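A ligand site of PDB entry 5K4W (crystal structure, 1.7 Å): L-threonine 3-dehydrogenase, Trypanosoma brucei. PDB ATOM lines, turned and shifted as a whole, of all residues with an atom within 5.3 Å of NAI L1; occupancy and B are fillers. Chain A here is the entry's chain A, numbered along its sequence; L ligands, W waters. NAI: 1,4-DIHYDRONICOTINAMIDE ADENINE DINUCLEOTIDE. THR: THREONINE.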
ATOM      1  N   GLY A   9     -32.860 -17.380 -11.021  1.00  0.00           N
ATOM      2  CA  GLY A   9     -31.553 -17.973 -10.772  1.00  0.00           C
ATOM      3  C   GLY A   9     -31.558 -18.979  -9.688  1.00  0.00           C
ATOM      4  O   GLY A   9     -30.633 -19.143  -8.868  1.00  0.00           O
ATOM      5  N   ALA A  10     -32.644 -19.710  -9.596  1.00  0.00           N
ATOM      6  CA  ALA A  10     -32.915 -20.437  -8.401  1.00  0.00           C
ATOM      7  C   ALA A  10     -32.188 -21.742  -8.229  1.00  0.00           C
ATOM      8  O   ALA A  10     -32.207 -22.298  -7.148  1.00  0.00           O
ATOM      9  CB  ALA A  10     -34.420 -20.653  -8.325  1.00  0.00           C
ATOM     10  N   LEU A  11     -31.601 -22.301  -9.286  1.00  0.00           N
ATOM     11  CA  LEU A  11     -30.937 -23.582  -9.168  1.00  0.00           C
ATOM     12  C   LEU A  11     -29.491 -23.568  -8.623  1.00  0.00           C
ATOM     13  O   LEU A  11     -28.881 -24.619  -8.358  1.00  0.00           O
ATOM     14  CB  LEU A  11     -30.921 -24.336 -10.504  1.00  0.00           C
ATOM     15  CG  LEU A  11     -32.222 -24.727 -11.154  1.00  0.00           C
ATOM     16  CD1 LEU A  11     -31.952 -25.555 -12.415  1.00  0.00           C
ATOM     17  CD2 LEU A  11     -33.135 -25.417 -10.218  1.00  0.00           C
ATOM     18  N   GLY A  12     -28.940 -22.393  -8.436  1.00  0.00           N
ATOM     19  CA  GLY A  12     -27.593 -22.259  -7.942  1.00  0.00           C
ATOM     20  C   GLY A  12     -27.402 -22.463  -6.477  1.00  0.00           C
ATOM     21  O   GLY A  12     -28.313 -22.921  -5.762  1.00  0.00           O
ATOM     22  N   GLN A  13     -26.223 -22.081  -5.999  1.00  0.00           N
ATOM     23  CA  GLN A  13     -25.885 -22.358  -4.608  1.00  0.00           C
ATOM     24  C   GLN A  13     -26.863 -21.660  -3.673  1.00  0.00           C
ATOM     25  O   GLN A  13     -27.429 -22.310  -2.765  1.00  0.00           O
ATOM     26  CB  GLN A  13     -24.478 -21.918  -4.308  1.00  0.00           C
ATOM     27  CG  GLN A  13     -24.063 -22.376  -2.931  1.00  0.00           C
ATOM     28  CD  GLN A  13     -22.819 -21.743  -2.444  1.00  0.00           C
ATOM     29  OE1 GLN A  13     -22.092 -21.099  -3.170  1.00  0.00           O
ATOM     30  NE2 GLN A  13     -22.536 -21.986  -1.215  1.00  0.00           N
ATOM     31  N   ILE A  14     -27.084 -20.368  -3.846  1.00  0.00           N
ATOM     32  CA  ILE A  14     -28.003 -19.711  -2.901  1.00  0.00           C
ATOM     33  C   ILE A  14     -29.470 -20.037  -3.165  1.00  0.00           C
ATOM     34  O   ILE A  14     -30.251 -20.306  -2.236  1.00  0.00           O
ATOM     35  CB  ILE A  14     -27.790 -18.188  -2.924  1.00  0.00           C
ATOM     36  CG1 ILE A  14     -26.367 -17.882  -2.390  1.00  0.00           C
ATOM     37  CG2 ILE A  14     -28.840 -17.495  -2.113  1.00  0.00           C
ATOM     38  CD1 ILE A  14     -26.034 -16.432  -2.290  1.00  0.00           C
ATOM     39  N   GLY A  15     -29.843 -20.041  -4.425  1.00  0.00           N
ATOM     40  CA  GLY A  15     -31.214 -20.246  -4.744  1.00  0.00           C
ATOM     41  C   GLY A  15     -31.763 -21.564  -4.315  1.00  0.00           C
ATOM     42  O   GLY A  15     -32.957 -21.673  -3.998  1.00  0.00           O
ATOM     43  N   ASP A  35     -35.122 -20.621 -13.511  1.00  0.00           N
ATOM     44  CA  ASP A  35     -33.714 -20.656 -13.873  1.00  0.00           C
ATOM     45  C   ASP A  35     -33.662 -20.933 -15.372  1.00  0.00           C
ATOM     46  O   ASP A  35     -34.629 -21.449 -15.962  1.00  0.00           O
ATOM     47  CB  ASP A  35     -32.978 -21.775 -13.131  1.00  0.00           C
ATOM     48  CG  ASP A  35     -31.494 -21.578 -13.058  1.00  0.00           C
ATOM     49  OD1 ASP A  35     -30.760 -21.863 -14.050  1.00  0.00           O
ATOM     50  OD2 ASP A  35     -31.002 -21.259 -11.970  1.00  0.00           O
ATOM     51  N   VAL A  36     -32.531 -20.576 -15.968  1.00  0.00           N
ATOM     52  CA  VAL A  36     -32.318 -20.732 -17.410  1.00  0.00           C
ATOM     53  C   VAL A  36     -32.141 -22.204 -17.725  1.00  0.00           C
ATOM     54  O   VAL A  36     -32.399 -22.609 -18.854  1.00  0.00           O
ATOM     55  CB  VAL A  36     -31.078 -19.925 -17.913  1.00  0.00           C
ATOM     56  CG1 VAL A  36     -29.798 -20.375 -17.230  1.00  0.00           C
ATOM     57  CG2 VAL A  36     -30.982 -19.983 -19.456  1.00  0.00           C
ATOM     58  N   VAL A  37     -31.696 -22.980 -16.744  1.00  0.00           N
ATOM     59  CA  VAL A  37     -31.495 -24.410 -16.905  1.00  0.00           C
ATOM     60  C   VAL A  37     -32.657 -25.162 -16.234  1.00  0.00           C
ATOM     61  O   VAL A  37     -33.279 -24.645 -15.289  1.00  0.00           O
ATOM     62  CB  VAL A  37     -30.162 -24.797 -16.160  1.00  0.00           C
ATOM     63  CG1 VAL A  37     -29.983 -26.287 -16.044  1.00  0.00           C
ATOM     64  CG2 VAL A  37     -28.968 -24.211 -16.949  1.00  0.00           C
ATOM     65  N   LEU A  54     -36.800 -20.201 -17.297  1.00  0.00           N
ATOM     66  CA  LEU A  54     -36.862 -18.811 -17.716  1.00  0.00           C
ATOM     67  C   LEU A  54     -35.428 -18.298 -17.909  1.00  0.00           C
ATOM     68  O   LEU A  54     -34.626 -18.350 -16.960  1.00  0.00           O
ATOM     69  CB  LEU A  54     -37.510 -17.888 -16.690  1.00  0.00           C
ATOM     70  CG  LEU A  54     -37.398 -16.331 -17.036  1.00  0.00           C
ATOM     71  CD1 LEU A  54     -38.156 -15.967 -18.289  1.00  0.00           C
ATOM     72  CD2 LEU A  54     -37.871 -15.532 -15.842  1.00  0.00           C
ATOM     73  N   ASP A  55     -35.143 -17.777 -19.084  1.00  0.00           N
ATOM     74  CA  ASP A  55     -33.884 -17.043 -19.339  1.00  0.00           C
ATOM     75  C   ASP A  55     -34.210 -15.567 -19.042  1.00  0.00           C
ATOM     76  O   ASP A  55     -35.004 -14.935 -19.736  1.00  0.00           O
ATOM     77  CB  ASP A  55     -33.479 -17.202 -20.809  1.00  0.00           C
ATOM     78  CG  ASP A  55     -32.179 -16.518 -21.145  1.00  0.00           C
ATOM     79  OD1 ASP A  55     -31.602 -15.726 -20.357  1.00  0.00           O
ATOM     80  OD2 ASP A  55     -31.728 -16.793 -22.291  1.00  0.00           O
ATOM     81  N   CYS A  56     -33.561 -14.975 -18.030  1.00  0.00           N
ATOM     82  CA  CYS A  56     -33.893 -13.623 -17.641  1.00  0.00           C
ATOM     83  C   CYS A  56     -33.359 -12.618 -18.648  1.00  0.00           C
ATOM     84  O   CYS A  56     -33.659 -11.435 -18.476  1.00  0.00           O
ATOM     85  CB  CYS A  56     -33.285 -13.255 -16.298  1.00  0.00           C
ATOM     86  SG  CYS A  56     -34.159 -14.051 -14.930  1.00  0.00           S
ATOM     87  N   LEU A  57     -32.606 -13.060 -19.639  1.00  0.00           N
ATOM     88  CA  LEU A  57     -32.243 -12.164 -20.766  1.00  0.00           C
ATOM     89  C   LEU A  57     -33.366 -12.030 -21.825  1.00  0.00           C
ATOM     90  O   LEU A  57     -33.301 -11.192 -22.775  1.00  0.00           O
ATOM     91  CB  LEU A  57     -30.951 -12.594 -21.422  1.00  0.00           C
ATOM     92  CG  LEU A  57     -29.632 -12.353 -20.693  1.00  0.00           C
ATOM     93  CD1 LEU A  57     -28.494 -12.986 -21.461  1.00  0.00           C
ATOM     94  CD2 LEU A  57     -29.407 -10.865 -20.445  1.00  0.00           C
ATOM     95  N   HIS A  76     -33.732 -11.664  -7.056  1.00  0.00           N
ATOM     96  CA  HIS A  76     -33.068 -11.842  -8.353  1.00  0.00           C
ATOM     97  C   HIS A  76     -31.644 -12.264  -8.232  1.00  0.00           C
ATOM     98  O   HIS A  76     -30.769 -11.456  -7.897  1.00  0.00           O
ATOM     99  CB  HIS A  76     -33.154 -10.529  -9.124  1.00  0.00           C
ATOM    100  CG  HIS A  76     -32.652 -10.643 -10.514  1.00  0.00           C
ATOM    101  ND1 HIS A  76     -33.292 -11.364 -11.505  1.00  0.00           N
ATOM    102  CD2 HIS A  76     -31.533 -10.142 -11.073  1.00  0.00           C
ATOM    103  CE1 HIS A  76     -32.633 -11.233 -12.643  1.00  0.00           C
ATOM    104  NE2 HIS A  76     -31.513 -10.546 -12.383  1.00  0.00           N
ATOM    105  N   LEU A  77     -31.381 -13.549  -8.493  1.00  0.00           N
ATOM    106  CA  LEU A  77     -30.068 -14.114  -8.197  1.00  0.00           C
ATOM    107  C   LEU A  77     -29.094 -14.404  -9.354  1.00  0.00           C
ATOM    108  O   LEU A  77     -27.919 -14.625  -9.058  1.00  0.00           O
ATOM    109  CB  LEU A  77     -30.263 -15.441  -7.407  1.00  0.00           C
ATOM    110  CG  LEU A  77     -31.107 -15.384  -6.183  1.00  0.00           C
ATOM    111  CD1 LEU A  77     -31.184 -16.821  -5.592  1.00  0.00           C
ATOM    112  CD2 LEU A  77     -30.575 -14.374  -5.148  1.00  0.00           C
ATOM    113  N   PRO A  78     -29.532 -14.299 -10.627  1.00  0.00           N
ATOM    114  CA  PRO A  78     -28.552 -14.696 -11.654  1.00  0.00           C
ATOM    115  C   PRO A  78     -27.381 -13.727 -11.680  1.00  0.00           C
ATOM    116  O   PRO A  78     -27.580 -12.519 -11.781  1.00  0.00           O
ATOM    117  CB  PRO A  78     -29.327 -14.641 -12.981  1.00  0.00           C
ATOM    118  CG  PRO A  78     -30.601 -14.005 -12.715  1.00  0.00           C
ATOM    119  CD  PRO A  78     -30.871 -13.961 -11.210  1.00  0.00           C
ATOM    120  N   ALA A  79     -26.177 -14.265 -11.681  1.00  0.00           N
ATOM    121  CA  ALA A  79     -24.979 -13.432 -11.919  1.00  0.00           C
ATOM    122  C   ALA A  79     -23.778 -14.350 -12.120  1.00  0.00           C
ATOM    123  O   ALA A  79     -23.723 -15.417 -11.548  1.00  0.00           O
ATOM    124  CB  ALA A  79     -24.660 -12.393 -10.819  1.00  0.00           C
ATOM    125  N   ILE A  80     -22.831 -13.854 -12.921  1.00  0.00           N
ATOM    126  CA  ILE A  80     -21.565 -14.522 -13.113  1.00  0.00           C
ATOM    127  C   ILE A  80     -20.574 -13.914 -12.114  1.00  0.00           C
ATOM    128  O   ILE A  80     -20.417 -12.719 -12.115  1.00  0.00           O
ATOM    129  CB  ILE A  80     -21.073 -14.299 -14.561  1.00  0.00           C
ATOM    130  CG1 ILE A  80     -22.166 -14.688 -15.575  1.00  0.00           C
ATOM    131  CG2 ILE A  80     -19.748 -15.018 -14.783  1.00  0.00           C
ATOM    132  CD1 ILE A  80     -22.640 -16.123 -15.459  1.00  0.00           C
ATOM    133  N   MET A  81     -19.917 -14.768 -11.317  1.00  0.00           N
ATOM    134  CA  MET A  81     -19.181 -14.309 -10.169  1.00  0.00           C
ATOM    135  C   MET A  81     -17.674 -14.147 -10.454  1.00  0.00           C
ATOM    136  O   MET A  81     -17.270 -14.091 -11.640  1.00  0.00           O
ATOM    137  CB  MET A  81     -19.448 -15.234  -8.972  1.00  0.00           C
ATOM    138  CG  MET A  81     -20.889 -15.171  -8.531  1.00  0.00           C
ATOM    139  SD  MET A  81     -21.345 -16.305  -7.222  1.00  0.00           S
ATOM    140  CE  MET A  81     -21.234 -17.861  -8.104  1.00  0.00           C
ATOM    141  N   ILE A  95     -25.163 -10.729 -18.340  1.00  0.00           N
ATOM    142  CA  ILE A  95     -26.048 -11.248 -17.386  1.00  0.00           C
ATOM    143  C   ILE A  95     -26.189 -10.290 -16.206  1.00  0.00           C
ATOM    144  O   ILE A  95     -27.328  -9.910 -15.800  1.00  0.00           O
ATOM    145  CB  ILE A  95     -25.586 -12.640 -16.873  1.00  0.00           C
ATOM    146  CG1 ILE A  95     -25.757 -13.657 -18.003  1.00  0.00           C
ATOM    147  CG2 ILE A  95     -26.341 -13.049 -15.631  1.00  0.00           C
ATOM    148  CD1 ILE A  95     -27.156 -14.052 -18.176  1.00  0.00           C
ATOM    149  N   THR A  99     -29.792  -8.474 -17.054  1.00  0.00           N
ATOM    150  CA  THR A  99     -30.902  -9.173 -16.360  1.00  0.00           C
ATOM    151  C   THR A  99     -31.364  -8.287 -15.143  1.00  0.00           C
ATOM    152  O   THR A  99     -32.541  -8.253 -14.781  1.00  0.00           O
ATOM    153  CB  THR A  99     -30.600 -10.576 -15.842  1.00  0.00           C
ATOM    154  OG1 THR A  99     -29.690 -10.601 -14.729  1.00  0.00           O
ATOM    155  CG2 THR A  99     -30.166 -11.503 -16.940  1.00  0.00           C
ATOM    156  N   PRO A 117     -28.733  -9.342  -4.569  1.00  0.00           N
ATOM    157  CA  PRO A 117     -27.577  -9.327  -3.701  1.00  0.00           C
ATOM    158  C   PRO A 117     -26.415  -8.587  -4.329  1.00  0.00           C
ATOM    159  O   PRO A 117     -26.167  -8.698  -5.536  1.00  0.00           O
ATOM    160  CB  PRO A 117     -27.236 -10.801  -3.505  1.00  0.00           C
ATOM    161  CG  PRO A 117     -27.692 -11.458  -4.794  1.00  0.00           C
ATOM    162  CD  PRO A 117     -28.923 -10.655  -5.192  1.00  0.00           C
ATOM    163  N   SER A 118     -25.675  -7.882  -3.484  1.00  0.00           N
ATOM    164  CA  SER A 118     -24.320  -7.430  -3.823  1.00  0.00           C
ATOM    165  C   SER A 118     -23.320  -8.362  -3.119  1.00  0.00           C
ATOM    166  O   SER A 118     -23.675  -9.485  -2.688  1.00  0.00           O
ATOM    167  CB  SER A 118     -24.143  -5.968  -3.453  1.00  0.00           C
ATOM    168  OG  SER A 118     -22.926  -5.501  -3.957  1.00  0.00           O
ATOM    169  N   THR A 119     -22.083  -7.916  -2.996  1.00  0.00           N
ATOM    170  CA  THR A 119     -21.035  -8.805  -2.640  1.00  0.00           C
ATOM    171  C   THR A 119     -19.852  -8.045  -2.122  1.00  0.00           C
ATOM    172  O   THR A 119     -19.642  -6.876  -2.431  1.00  0.00           O
ATOM    173  CB  THR A 119     -20.585  -9.629  -3.870  1.00  0.00           C
ATOM    174  OG1 THR A 119     -19.387 -10.344  -3.548  1.00  0.00           O
ATOM    175  CG2 THR A 119     -20.367  -8.820  -5.072  1.00  0.00           C
ATOM    176  N   TYR A 144     -16.925  -8.639 -12.342  1.00  0.00           N
ATOM    177  CA  TYR A 144     -18.068  -8.999 -11.485  1.00  0.00           C
ATOM    178  C   TYR A 144     -18.352  -7.869 -10.444  1.00  0.00           C
ATOM    179  O   TYR A 144     -19.499  -7.353 -10.360  1.00  0.00           O
ATOM    180  CB  TYR A 144     -17.768 -10.247 -10.735  1.00  0.00           C
ATOM    181  CG  TYR A 144     -18.681 -10.639  -9.610  1.00  0.00           C
ATOM    182  CD1 TYR A 144     -20.052 -10.790  -9.757  1.00  0.00           C
ATOM    183  CD2 TYR A 144     -18.127 -10.976  -8.396  1.00  0.00           C
ATOM    184  CE1 TYR A 144     -20.853 -11.266  -8.706  1.00  0.00           C
ATOM    185  CE2 TYR A 144     -18.865 -11.491  -7.348  1.00  0.00           C
ATOM    186  CZ  TYR A 144     -20.204 -11.611  -7.485  1.00  0.00           C
ATOM    187  OH  TYR A 144     -20.943 -12.115  -6.503  1.00  0.00           O
ATOM    188  N   LYS A 148     -21.550  -5.269  -9.952  1.00  0.00           N
ATOM    189  CA  LYS A 148     -22.303  -5.194  -8.693  1.00  0.00           C
ATOM    190  C   LYS A 148     -22.326  -3.795  -8.114  1.00  0.00           C
ATOM    191  O   LYS A 148     -23.343  -3.443  -7.528  1.00  0.00           O
ATOM    192  CB  LYS A 148     -21.833  -6.246  -7.720  1.00  0.00           C
ATOM    193  CG  LYS A 148     -22.144  -7.687  -8.108  1.00  0.00           C
ATOM    194  CD  LYS A 148     -23.609  -7.994  -7.986  1.00  0.00           C
ATOM    195  CE  LYS A 148     -23.978  -9.471  -8.104  1.00  0.00           C
ATOM    196  NZ  LYS A 148     -25.423  -9.621  -8.016  1.00  0.00           N
ATOM    197  N   LEU A 171     -23.067  -9.602   0.383  1.00  0.00           N
ATOM    198  CA  LEU A 171     -22.852 -10.901   0.995  1.00  0.00           C
ATOM    199  C   LEU A 171     -21.351 -11.212   1.006  1.00  0.00           C
ATOM    200  O   LEU A 171     -20.636 -10.868   0.072  1.00  0.00           O
ATOM    201  CB  LEU A 171     -23.547 -11.969   0.152  1.00  0.00           C
ATOM    202  CG  LEU A 171     -25.071 -11.989   0.280  1.00  0.00           C
ATOM    203  CD1 LEU A 171     -25.677 -13.001  -0.681  1.00  0.00           C
ATOM    204  CD2 LEU A 171     -25.504 -12.219   1.730  1.00  0.00           C
ATOM    205  N   PRO A 172     -20.909 -11.908   2.049  1.00  0.00           N
ATOM    206  CA  PRO A 172     -19.600 -12.473   2.176  1.00  0.00           C
ATOM    207  C   PRO A 172     -19.581 -13.772   1.389  1.00  0.00           C
ATOM    208  O   PRO A 172     -20.574 -14.170   0.794  1.00  0.00           O
ATOM    209  CB  PRO A 172     -19.472 -12.674   3.651  1.00  0.00           C
ATOM    210  CG  PRO A 172     -20.820 -13.067   4.075  1.00  0.00           C
ATOM    211  CD  PRO A 172     -21.760 -12.247   3.191  1.00  0.00           C
ATOM    212  N   GLY A 173     -18.492 -14.501   1.444  1.00  0.00           N
ATOM    213  CA  GLY A 173     -18.519 -15.850   0.890  1.00  0.00           C
ATOM    214  C   GLY A 173     -19.461 -16.769   1.613  1.00  0.00           C
ATOM    215  O   GLY A 173     -19.482 -16.827   2.842  1.00  0.00           O
ATOM    216  N   ILE A 174     -20.306 -17.458   0.843  1.00  0.00           N
ATOM    217  CA  ILE A 174     -21.372 -18.277   1.432  1.00  0.00           C
ATOM    218  C   ILE A 174     -20.956 -19.748   1.311  1.00  0.00           C
ATOM    219  O   ILE A 174     -20.585 -20.260   0.231  1.00  0.00           O
ATOM    220  CB  ILE A 174     -22.759 -18.028   0.760  1.00  0.00           C
ATOM    221  CG1 ILE A 174     -23.130 -16.541   0.793  1.00  0.00           C
ATOM    222  CG2 ILE A 174     -23.806 -18.905   1.411  1.00  0.00           C
ATOM    223  CD1 ILE A 174     -23.078 -15.895   2.166  1.00  0.00           C
ATOM    224  N   LEU A 180     -23.257 -27.281  -5.457  1.00  0.00           N
ATOM    225  CA  LEU A 180     -21.859 -26.844  -5.618  1.00  0.00           C
ATOM    226  C   LEU A 180     -21.770 -25.432  -6.141  1.00  0.00           C
ATOM    227  O   LEU A 180     -22.715 -24.955  -6.829  1.00  0.00           O
ATOM    228  CB  LEU A 180     -21.070 -27.769  -6.560  1.00  0.00           C
ATOM    229  CG  LEU A 180     -20.761 -29.181  -5.987  1.00  0.00           C
ATOM    230  CD1 LEU A 180     -20.100 -30.060  -7.061  1.00  0.00           C
ATOM    231  CD2 LEU A 180     -19.821 -29.118  -4.838  1.00  0.00           C
ATOM    232  N   PRO A 181     -20.662 -24.752  -5.781  1.00  0.00           N
ATOM    233  CA  PRO A 181     -20.673 -23.278  -6.064  1.00  0.00           C
ATOM    234  C   PRO A 181     -20.380 -22.951  -7.493  1.00  0.00           C
ATOM    235  O   PRO A 181     -19.925 -23.832  -8.240  1.00  0.00           O
ATOM    236  CB  PRO A 181     -19.541 -22.764  -5.207  1.00  0.00           C
ATOM    237  CG  PRO A 181     -18.649 -23.972  -4.906  1.00  0.00           C
ATOM    238  CD  PRO A 181     -19.544 -25.153  -4.904  1.00  0.00           C
ATOM    239  N   GLY A 182     -20.619 -21.691  -7.855  1.00  0.00           N
ATOM    240  CA  GLY A 182     -20.671 -21.305  -9.333  1.00  0.00           C
ATOM    241  C   GLY A 182     -19.454 -20.633  -9.936  1.00  0.00           C
ATOM    242  O   GLY A 182     -19.567 -20.067 -11.066  1.00  0.00           O
ATOM    243  N   THR A 186     -14.224 -17.784  -3.429  1.00  0.00           N
ATOM    244  CA  THR A 186     -14.368 -18.429  -2.128  1.00  0.00           C
ATOM    245  C   THR A 186     -14.726 -19.905  -2.227  1.00  0.00           C
ATOM    246  O   THR A 186     -14.862 -20.586  -1.228  1.00  0.00           O
ATOM    247  CB  THR A 186     -15.465 -17.756  -1.315  1.00  0.00           C
ATOM    248  OG1 THR A 186     -16.682 -17.808  -2.082  1.00  0.00           O
ATOM    249  CG2 THR A 186     -15.139 -16.322  -1.023  1.00  0.00           C
HETATM  250  PA  NAI L   1     -24.707 -19.765  -8.824  1.00  0.00           P
HETATM  251  O1A NAI L   1     -24.495 -21.009  -7.904  1.00  0.00           O
HETATM  252  O2A NAI L   1     -23.709 -19.561  -9.947  1.00  0.00           O
HETATM  253  O5B NAI L   1     -26.241 -19.644  -9.407  1.00  0.00           O
HETATM  254  C5B NAI L   1     -26.477 -18.716 -10.474  1.00  0.00           C
HETATM  255  C4B NAI L   1     -27.766 -19.333 -11.041  1.00  0.00           C
HETATM  256  O4B NAI L   1     -28.257 -18.405 -12.049  1.00  0.00           O
HETATM  257  C3B NAI L   1     -27.692 -20.577 -11.843  1.00  0.00           C
HETATM  258  O3B NAI L   1     -28.366 -21.699 -11.404  1.00  0.00           O
HETATM  259  C2B NAI L   1     -27.658 -20.240 -13.242  1.00  0.00           C
HETATM  260  O2B NAI L   1     -28.180 -21.301 -14.087  1.00  0.00           O
HETATM  261  C1B NAI L   1     -28.629 -19.067 -13.189  1.00  0.00           C
HETATM  262  N9A NAI L   1     -28.545 -18.214 -14.410  1.00  0.00           N
HETATM  263  C8A NAI L   1     -27.441 -17.763 -15.070  1.00  0.00           C
HETATM  264  N7A NAI L   1     -27.889 -17.028 -16.129  1.00  0.00           N
HETATM  265  C5A NAI L   1     -29.199 -16.926 -16.031  1.00  0.00           C
HETATM  266  C6A NAI L   1     -30.142 -16.329 -16.860  1.00  0.00           C
HETATM  267  N6A NAI L   1     -29.737 -15.724 -17.961  1.00  0.00           N
HETATM  268  N1A NAI L   1     -31.469 -16.416 -16.597  1.00  0.00           N
HETATM  269  C2A NAI L   1     -31.847 -17.123 -15.472  1.00  0.00           C
HETATM  270  N3A NAI L   1     -30.895 -17.800 -14.673  1.00  0.00           N
HETATM  271  C4A NAI L   1     -29.594 -17.661 -14.971  1.00  0.00           C
HETATM  272  O3  NAI L   1     -24.603 -18.402  -7.975  1.00  0.00           O
HETATM  273  PN  NAI L   1     -24.935 -18.252  -6.437  1.00  0.00           P
HETATM  274  O1N NAI L   1     -26.199 -18.973  -6.051  1.00  0.00           O
HETATM  275  O2N NAI L   1     -23.724 -18.520  -5.583  1.00  0.00           O
HETATM  276  O5D NAI L   1     -25.285 -16.621  -6.433  1.00  0.00           O
HETATM  277  C5D NAI L   1     -26.610 -16.098  -6.620  1.00  0.00           C
HETATM  278  C4D NAI L   1     -26.240 -14.683  -6.410  1.00  0.00           C
HETATM  279  O4D NAI L   1     -25.891 -14.285  -5.100  1.00  0.00           O
HETATM  280  C3D NAI L   1     -25.544 -13.749  -7.302  1.00  0.00           C
HETATM  281  O3D NAI L   1     -26.096 -12.550  -7.675  1.00  0.00           O
HETATM  282  C2D NAI L   1     -24.246 -13.744  -6.770  1.00  0.00           C
HETATM  283  O2D NAI L   1     -23.509 -12.551  -7.112  1.00  0.00           O
HETATM  284  C1D NAI L   1     -24.680 -13.751  -5.301  1.00  0.00           C
HETATM  285  N1N NAI L   1     -23.765 -13.707  -4.171  1.00  0.00           N
HETATM  286  C2N NAI L   1     -23.244 -14.978  -4.023  1.00  0.00           C
HETATM  287  C3N NAI L   1     -22.242 -15.284  -3.102  1.00  0.00           C
HETATM  288  C7N NAI L   1     -21.711 -16.594  -2.807  1.00  0.00           C
HETATM  289  O7N NAI L   1     -20.743 -16.728  -2.020  1.00  0.00           O
HETATM  290  N7N NAI L   1     -22.215 -17.709  -3.430  1.00  0.00           N
HETATM  291  C4N NAI L   1     -21.853 -14.163  -2.258  1.00  0.00           C
HETATM  292  C5N NAI L   1     -22.159 -12.871  -2.765  1.00  0.00           C
HETATM  293  C6N NAI L   1     -23.083 -12.608  -3.722  1.00  0.00           C
HETATM  294  N   THR L   2     -18.533 -16.419  -3.873  1.00  0.00           N
HETATM  295  CA  THR L   2     -18.495 -15.173  -4.680  1.00  0.00           C
HETATM  296  C   THR L   2     -17.123 -15.031  -5.258  1.00  0.00           C
HETATM  297  O   THR L   2     -17.061 -14.392  -6.298  1.00  0.00           O
HETATM  298  CB  THR L   2     -18.980 -14.010  -3.835  1.00  0.00           C
HETATM  299  OG1 THR L   2     -19.162 -12.848  -4.626  1.00  0.00           O
HETATM  300  CG2 THR L   2     -18.048 -13.801  -2.625  1.00  0.00           C
HETATM  301  OXT THR L   2     -16.193 -15.673  -4.687  1.00  0.00           O
HETATM  302  O   HOH W   1     -23.798 -21.182 -12.122  1.00  0.00           O
HETATM  303  O   HOH W   2     -21.671 -20.093  -5.754  1.00  0.00           O
HETATM  304  O   HOH W   3     -23.049 -17.824 -11.899  1.00  0.00           O
HETATM  305  O   HOH W   4     -24.480 -18.985 -13.671  1.00  0.00           O
HETATM  306  O   HOH W   5     -28.175 -11.182  -8.991  1.00  0.00           O
HETATM  307  O   HOH W   6     -27.264 -24.011 -12.399  1.00  0.00           O
HETATM  308  O   HOH W   7     -26.511 -21.677 -16.380  1.00  0.00           O
HETATM  309  O   HOH W   8     -27.836 -17.051 -20.001  1.00  0.00           O
HETATM  310  O   HOH W   9     -34.834 -17.351 -14.102  1.00  0.00           O
HETATM  311  O   HOH W  10     -28.738 -19.360  -6.907  1.00  0.00           O
HETATM  312  O   HOH W  11     -23.760 -23.289  -8.778  1.00  0.00           O
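Water W11 lies within hydrogen-bond range of an oxygen (O1A) of NAI L1 (2.6 Å) and the backbone carbonyl oxygen of Leu 180 (2.8 Å).
Water W2 lies within hydrogen-bond range of O2N of NAI L1 (2.6 Å), OE1 of Gln 13 (2.8 Å) and N of Gly 182 (2.8 Å).
Water W3 lies within hydrogen-bond range of O of Ala 79 (2.5 Å) and O2A of NAI L1 (2.7 Å).
Water W10 lies within hydrogen-bond range of an oxygen (O1N) of NAI L1 (2.7 Å), the backbone carbonyl oxygen of Gly 9 (2.7 Å), the backbone NH of Gly 15 (2.8 Å) and the backbone NH of Gly 12 (3.4 Å).
Water W9 lies within hydrogen-bond range of the backbone carbonyl oxygen (O) of Leu 54, the backbone NH (N) of Asp 35 and the side-chain sulfur (SG) of Cys 56.
The side-chain sulfur (SD) of Met 81 sits close to an oxygen (O2N) of NAI L1 (3.6 Å).
Gly 9 touches NAI L1 (CA to O4B, 3.6 Å).
Leu 11 touches NAI L1.
Leu 54 touches NAI L1 (O to C2A, 3.4 Å).
Pro 78 touches NAI L1.
CB of Ala 79 touches O3D of NAI L1, at 3.5 Å.
Ile 95 touches NAI L1.
CG of Pro 117 touches O4D of NAI L1, at 3.4 Å.
Ser 118 touches NAI L1.
Thr 119 touches NAI L1.
Leu 171 touches NAI L1.
Pro 172 touches NAI L1 (O to C4N, 3.3 Å).
Gly 173 touches NAI L1.
CA of Gly 182 touches O2A of NAI L1 (3.6 Å).
Hydrophobic or aromatic side chains within 4 Å of NAI L1: Leu 11, Ile 14, Val 36, Leu 77, Pro 78, Ala 79, Met 81, Ile 95, Pro 117, Tyr 144, Leu 171 and Ile 174.
Of the 35 residues printed, 25 come within 4 Å of NAI L1.
The nearest printed residue that does not touch NAI L1 is Gly 15 (4.1 Å).
N of THR L2 is in hydrogen-bond range of O7N of NAI L1 (2.9 Å).
OG1 of Thr 99 is in hydrogen-bond range of O of Ile 95 (2.7 Å).
The side-chain carboxylate (OD1) of Asp 35 is in hydrogen-bond range of the backbone NH (N) of Val 37.
O of Ile 174 is in hydrogen-bond range of NE2 of Gln 13 (3.0 Å).
NZ of Lys 148 sits at hydrogen-bond distance from O of Pro 117 (2.7 Å).
The side-chain carboxylate (OD2) of Asp 35 lies within hydrogen-bond range of the backbone NH (N) of Ala 10 (3.3 Å).
O of Ser 118 sits at hydrogen-bond distance from N of Leu 171 (3.1 Å).
The backbone NH of Leu 11 is in hydrogen-bond range of the side-chain carboxylate of Asp 35 (2.9 Å).
The backbone NH (N) of Val 36 is in hydrogen-bond range of the backbone carbonyl oxygen (O) of Leu 54, at 3.2 Å.
The side-chain hydroxyl (OG1) of Thr 186 lies within hydrogen-bond range of a nitrogen (N) of THR L2, at 2.9 Å.
The backbone NH (N) of Cys 56 lies within hydrogen-bond range of a nitrogen (N1A) of NAI L1, 2.9 Å away.
N of Gly 12 is in hydrogen-bond range of O3B of NAI L1.
The backbone NH (N) of Val 36 is in hydrogen-bond range of a nitrogen (N3A) of NAI L1 (3.5 Å).
The side-chain hydroxyl (OG1) of Thr 119 lies within hydrogen-bond range of an oxygen (OG1) of THR L2 (2.7 Å).
The backbone NH (N) of Ile 174 lies within hydrogen-bond range of an oxygen (O7N) of NAI L1, at 3.0 Å.
An oxygen (O2D) of NAI L1 sits at hydrogen-bond distance from the side-chain hydroxyl (OH) of Tyr 144, 2.7 Å away.
The side-chain carboxylate (OD1) of Asp 35 is in hydrogen-bond range of an oxygen (O2B) of NAI L1.
The side-chain amide oxygen of Gln 13 is in hydrogen-bond range of a nitrogen (N7N) of NAI L1 (3.4 Å).
An oxygen (O3D) of NAI L1 lies close to the backbone carbonyl oxygen of Leu 77, at 3.1 Å.
N6A of NAI L1 sits at hydrogen-bond distance from OD1 of Asp 55.
N of Gln 13 lies within hydrogen-bond range of O1A of NAI L1 (2.8 Å).
The side-chain hydroxyl (OH) of Tyr 144 lies within hydrogen-bond range of an oxygen (OG1) of THR L2 (2.7 Å).
An oxygen (O1N) of NAI L1 lies within hydrogen-bond range of the backbone NH of Ile 14, at 2.8 Å.
NZ of Lys 148 sits at hydrogen-bond distance from O3D of NAI L1.
The backbone NH of Thr 186 is in hydrogen-bond range of an oxygen (OXT) of THR L2 (3.1 Å).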
